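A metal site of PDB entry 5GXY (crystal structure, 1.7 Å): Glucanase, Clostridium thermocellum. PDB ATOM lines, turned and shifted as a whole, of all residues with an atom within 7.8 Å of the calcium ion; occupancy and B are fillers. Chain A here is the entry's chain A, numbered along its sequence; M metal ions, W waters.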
ATOM      1  N   THR A 461      13.696  -7.685 -33.706  1.00  0.00           N
ATOM      2  CA  THR A 461      12.573  -8.573 -33.990  1.00  0.00           C
ATOM      3  C   THR A 461      12.694  -8.986 -35.458  1.00  0.00           C
ATOM      4  O   THR A 461      12.867  -8.119 -36.314  1.00  0.00           O
ATOM      5  CB  THR A 461      11.233  -7.826 -33.820  1.00  0.00           C
ATOM      6  OG1 THR A 461      11.037  -7.470 -32.447  1.00  0.00           O
ATOM      7  CG2 THR A 461      10.081  -8.710 -34.256  1.00  0.00           C
ATOM      8  N   TYR A 486       3.330  -2.135 -37.064  1.00  0.00           N
ATOM      9  CA  TYR A 486       3.403  -0.993 -36.141  1.00  0.00           C
ATOM     10  C   TYR A 486       4.226  -1.300 -34.905  1.00  0.00           C
ATOM     11  O   TYR A 486       4.112  -2.378 -34.315  1.00  0.00           O
ATOM     12  CB  TYR A 486       2.002  -0.607 -35.668  1.00  0.00           C
ATOM     13  CG  TYR A 486       1.083  -0.151 -36.772  1.00  0.00           C
ATOM     14  CD1 TYR A 486       1.075   1.169 -37.203  1.00  0.00           C
ATOM     15  CD2 TYR A 486       0.218  -1.063 -37.389  1.00  0.00           C
ATOM     16  CE1 TYR A 486       0.235   1.593 -38.232  1.00  0.00           C
ATOM     17  CE2 TYR A 486      -0.642  -0.649 -38.407  1.00  0.00           C
ATOM     18  CZ  TYR A 486      -0.628   0.671 -38.817  1.00  0.00           C
ATOM     19  OH  TYR A 486      -1.477   1.067 -39.822  1.00  0.00           O
ATOM     20  N   MET A 487       5.010  -0.308 -34.502  1.00  0.00           N
ATOM     21  CA  MET A 487       5.899  -0.415 -33.349  1.00  0.00           C
ATOM     22  C   MET A 487       5.706   0.793 -32.441  1.00  0.00           C
ATOM     23  O   MET A 487       5.305   1.853 -32.900  1.00  0.00           O
ATOM     24  CB  MET A 487       7.345  -0.386 -33.831  1.00  0.00           C
ATOM     25  CG  MET A 487       7.768  -1.623 -34.599  1.00  0.00           C
ATOM     26  SD  MET A 487       9.197  -1.206 -35.622  1.00  0.00           S
ATOM     27  CE  MET A 487       8.424  -0.307 -36.978  1.00  0.00           C
ATOM     28  N   ASP A 488       6.036   0.636 -31.165  1.00  0.00           N
ATOM     29  CA  ASP A 488       6.118   1.738 -30.227  1.00  0.00           C
ATOM     30  C   ASP A 488       7.602   1.893 -29.948  1.00  0.00           C
ATOM     31  O   ASP A 488       8.244   0.965 -29.478  1.00  0.00           O
ATOM     32  CB  ASP A 488       5.392   1.377 -28.942  1.00  0.00           C
ATOM     33  CG  ASP A 488       5.342   2.524 -27.953  1.00  0.00           C
ATOM     34  OD1 ASP A 488       6.263   3.371 -27.951  1.00  0.00           O
ATOM     35  OD2 ASP A 488       4.369   2.549 -27.183  1.00  0.00           O
ATOM     36  N   LEU A 489       8.163   3.052 -30.285  1.00  0.00           N
ATOM     37  CA  LEU A 489       9.585   3.296 -30.118  1.00  0.00           C
ATOM     38  C   LEU A 489       9.937   4.108 -28.867  1.00  0.00           C
ATOM     39  O   LEU A 489      11.034   4.668 -28.777  1.00  0.00           O
ATOM     40  CB  LEU A 489      10.138   3.967 -31.374  1.00  0.00           C
ATOM     41  CG  LEU A 489       9.987   3.162 -32.671  1.00  0.00           C
ATOM     42  CD1 LEU A 489      10.659   3.924 -33.804  1.00  0.00           C
ATOM     43  CD2 LEU A 489      10.588   1.768 -32.540  1.00  0.00           C
ATOM     44  N   THR A 490       9.035   4.109 -27.882  1.00  0.00           N
ATOM     45  CA  THR A 490       9.276   4.826 -26.622  1.00  0.00           C
ATOM     46  C   THR A 490      10.585   4.441 -25.949  1.00  0.00           C
ATOM     47  O   THR A 490      11.332   5.328 -25.514  1.00  0.00           O
ATOM     48  CB  THR A 490       8.136   4.614 -25.607  1.00  0.00           C
ATOM     49  OG1 THR A 490       6.902   5.097 -26.148  1.00  0.00           O
ATOM     50  CG2 THR A 490       8.421   5.367 -24.310  1.00  0.00           C
ATOM     51  N   GLU A 491      10.869   3.142 -25.867  1.00  0.00           N
ATOM     52  CA  GLU A 491      12.088   2.632 -25.232  1.00  0.00           C
ATOM     53  C   GLU A 491      13.359   3.012 -25.992  1.00  0.00           C
ATOM     54  O   GLU A 491      14.435   3.122 -25.395  1.00  0.00           O
ATOM     55  CB  GLU A 491      12.001   1.108 -25.051  1.00  0.00           C
ATOM     56  CG  GLU A 491      12.224   0.276 -26.316  1.00  0.00           C
ATOM     57  CD  GLU A 491      10.975   0.026 -27.163  1.00  0.00           C
ATOM     58  OE1 GLU A 491       9.881   0.533 -26.817  1.00  0.00           O
ATOM     59  OE2 GLU A 491      11.108  -0.685 -28.182  1.00  0.00           O
ATOM     60  N   VAL A 492      13.230   3.214 -27.299  1.00  0.00           N
ATOM     61  CA  VAL A 492      14.347   3.641 -28.129  1.00  0.00           C
ATOM     62  C   VAL A 492      14.779   5.035 -27.712  1.00  0.00           C
ATOM     63  O   VAL A 492      15.943   5.274 -27.390  1.00  0.00           O
ATOM     64  CB  VAL A 492      13.976   3.647 -29.620  1.00  0.00           C
ATOM     65  CG1 VAL A 492      15.137   4.138 -30.477  1.00  0.00           C
ATOM     66  CG2 VAL A 492      13.536   2.256 -30.058  1.00  0.00           C
ATOM     67  N   ASN A 526       4.722   8.166 -30.157  1.00  0.00           N
ATOM     68  CA  ASN A 526       5.895   7.321 -30.369  1.00  0.00           C
ATOM     69  C   ASN A 526       5.598   6.071 -31.203  1.00  0.00           C
ATOM     70  O   ASN A 526       6.387   5.126 -31.222  1.00  0.00           O
ATOM     71  CB  ASN A 526       6.541   6.924 -29.036  1.00  0.00           C
ATOM     72  CG  ASN A 526       7.127   8.105 -28.307  1.00  0.00           C
ATOM     73  OD1 ASN A 526       7.417   9.138 -28.908  1.00  0.00           O
ATOM     74  ND2 ASN A 526       7.322   7.968 -26.996  1.00  0.00           N
ATOM     75  N   PHE A 564      17.955  -2.307 -25.151  1.00  0.00           N
ATOM     76  CA  PHE A 564      16.701  -1.588 -24.935  1.00  0.00           C
ATOM     77  C   PHE A 564      15.521  -2.097 -25.759  1.00  0.00           C
ATOM     78  O   PHE A 564      14.369  -1.908 -25.356  1.00  0.00           O
ATOM     79  CB  PHE A 564      16.886  -0.085 -25.151  1.00  0.00           C
ATOM     80  CG  PHE A 564      17.290   0.297 -26.547  1.00  0.00           C
ATOM     81  CD1 PHE A 564      16.350   0.366 -27.576  1.00  0.00           C
ATOM     82  CD2 PHE A 564      18.597   0.642 -26.839  1.00  0.00           C
ATOM     83  CE1 PHE A 564      16.713   0.739 -28.861  1.00  0.00           C
ATOM     84  CE2 PHE A 564      18.979   1.027 -28.115  1.00  0.00           C
ATOM     85  CZ  PHE A 564      18.036   1.075 -29.131  1.00  0.00           C
ATOM     86  N   TRP A 565      15.802  -2.725 -26.886  1.00  0.00           N
ATOM     87  CA  TRP A 565      14.732  -3.138 -27.819  1.00  0.00           C
ATOM     88  C   TRP A 565      13.610  -3.886 -27.102  1.00  0.00           C
ATOM     89  O   TRP A 565      13.851  -4.902 -26.440  1.00  0.00           O
ATOM     90  CB  TRP A 565      15.299  -3.991 -28.952  1.00  0.00           C
ATOM     91  CG  TRP A 565      14.278  -4.295 -30.029  1.00  0.00           C
ATOM     92  CD1 TRP A 565      13.684  -5.504 -30.271  1.00  0.00           C
ATOM     93  CD2 TRP A 565      13.717  -3.371 -30.959  1.00  0.00           C
ATOM     94  NE1 TRP A 565      12.798  -5.375 -31.315  1.00  0.00           N
ATOM     95  CE2 TRP A 565      12.810  -4.083 -31.763  1.00  0.00           C
ATOM     96  CE3 TRP A 565      13.915  -2.000 -31.210  1.00  0.00           C
ATOM     97  CZ2 TRP A 565      12.076  -3.476 -32.790  1.00  0.00           C
ATOM     98  CZ3 TRP A 565      13.198  -1.404 -32.226  1.00  0.00           C
ATOM     99  CH2 TRP A 565      12.297  -2.140 -33.006  1.00  0.00           C
ATOM    100  N   ASP A 566      12.384  -3.375 -27.203  1.00  0.00           N
ATOM    101  CA  ASP A 566      11.252  -3.975 -26.514  1.00  0.00           C
ATOM    102  C   ASP A 566      10.066  -4.144 -27.460  1.00  0.00           C
ATOM    103  O   ASP A 566       9.326  -3.191 -27.743  1.00  0.00           O
ATOM    104  CB  ASP A 566      10.870  -3.138 -25.294  1.00  0.00           C
ATOM    105  CG  ASP A 566       9.681  -3.707 -24.550  1.00  0.00           C
ATOM    106  OD1 ASP A 566       9.319  -4.885 -24.749  1.00  0.00           O
ATOM    107  OD2 ASP A 566       9.089  -2.944 -23.749  1.00  0.00           O
ATOM    108  N   PRO A 567       9.901  -5.365 -27.982  1.00  0.00           N
ATOM    109  CA  PRO A 567       8.778  -5.525 -28.907  1.00  0.00           C
ATOM    110  C   PRO A 567       7.457  -5.732 -28.189  1.00  0.00           C
ATOM    111  O   PRO A 567       6.424  -5.733 -28.859  1.00  0.00           O
ATOM    112  CB  PRO A 567       9.149  -6.789 -29.683  1.00  0.00           C
ATOM    113  CG  PRO A 567       9.919  -7.605 -28.700  1.00  0.00           C
ATOM    114  CD  PRO A 567      10.686  -6.604 -27.854  1.00  0.00           C
ATOM    115  N   THR A 568       7.483  -5.889 -26.870  1.00  0.00           N
ATOM    116  CA  THR A 568       6.259  -6.218 -26.125  1.00  0.00           C
ATOM    117  C   THR A 568       5.273  -5.055 -26.067  1.00  0.00           C
ATOM    118  O   THR A 568       4.100  -5.246 -25.760  1.00  0.00           O
ATOM    119  CB  THR A 568       6.529  -6.815 -24.717  1.00  0.00           C
ATOM    120  OG1 THR A 568       6.987  -5.788 -23.841  1.00  0.00           O
ATOM    121  CG2 THR A 568       7.573  -7.944 -24.777  1.00  0.00           C
ATOM    122  N   ASN A 569       5.730  -3.850 -26.382  1.00  0.00           N
ATOM    123  CA  ASN A 569       4.796  -2.727 -26.499  1.00  0.00           C
ATOM    124  C   ASN A 569       4.441  -2.379 -27.950  1.00  0.00           C
ATOM    125  O   ASN A 569       3.783  -1.369 -28.208  1.00  0.00           O
ATOM    126  CB  ASN A 569       5.288  -1.514 -25.706  1.00  0.00           C
ATOM    127  CG  ASN A 569       6.568  -0.900 -26.242  1.00  0.00           C
ATOM    128  OD1 ASN A 569       7.117  -1.356 -27.252  1.00  0.00           O
ATOM    129  ND2 ASN A 569       7.053   0.137 -25.569  1.00  0.00           N
ATOM    130  N   ASP A 570       4.848  -3.226 -28.886  1.00  0.00           N
ATOM    131  CA  ASP A 570       4.589  -2.961 -30.294  1.00  0.00           C
ATOM    132  C   ASP A 570       3.228  -3.537 -30.712  1.00  0.00           C
ATOM    133  O   ASP A 570       2.940  -4.719 -30.486  1.00  0.00           O
ATOM    134  CB  ASP A 570       5.689  -3.528 -31.187  1.00  0.00           C
ATOM    135  CG  ASP A 570       7.061  -2.903 -30.916  1.00  0.00           C
ATOM    136  OD1 ASP A 570       7.209  -1.911 -30.155  1.00  0.00           O
ATOM    137  OD2 ASP A 570       8.037  -3.463 -31.490  1.00  0.00           O
ATOM    138  N   PHE A 571       2.408  -2.684 -31.308  1.00  0.00           N
ATOM    139  CA  PHE A 571       1.056  -3.060 -31.719  1.00  0.00           C
ATOM    140  C   PHE A 571       1.001  -4.328 -32.565  1.00  0.00           C
ATOM    141  O   PHE A 571       0.166  -5.208 -32.339  1.00  0.00           O
ATOM    142  CB  PHE A 571       0.430  -1.897 -32.488  1.00  0.00           C
ATOM    143  CG  PHE A 571      -0.980  -2.134 -32.968  1.00  0.00           C
ATOM    144  CD1 PHE A 571      -2.061  -1.828 -32.154  1.00  0.00           C
ATOM    145  CD2 PHE A 571      -1.206  -2.612 -34.256  1.00  0.00           C
ATOM    146  CE1 PHE A 571      -3.366  -2.014 -32.627  1.00  0.00           C
ATOM    147  CE2 PHE A 571      -2.497  -2.794 -34.729  1.00  0.00           C
ATOM    148  CZ  PHE A 571      -3.579  -2.488 -33.915  1.00  0.00           C
HETATM  149 CA    CA M   1       8.889  -1.129 -28.737  1.00  0.00          CA
HETATM  150  O   HOH W   1      10.041  -1.882 -30.734  1.00  0.00           O
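OD1 of Asp 488 is in hydrogen-bond range of OG1 of Thr 490 (2.6 Å).
OD1 of Asp 566 sits at hydrogen-bond distance from OG1 of Thr 568, at 2.7 Å.
The calcium ion is bound by the backbone carbonyl oxygen (O) of Asp 488 (2.3 Å), the side-chain amide oxygen (OD1) of Asn 569 (2.3 Å), the side-chain carboxylate (OE2) of Glu 491 (2.3 Å), the backbone carbonyl oxygen (O) of Asp 566 (2.3 Å), the side-chain carboxylate (OD1) of Asp 570 (2.3 Å), water W1 (2.4 Å) and the side-chain carboxylate (OE1) of Glu 491 (2.7 Å).
Five residues have an atom within 4 Å of the calcium ion: Asp 488, Glu 491, Asp 566, Asn 569 and Asp 570.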
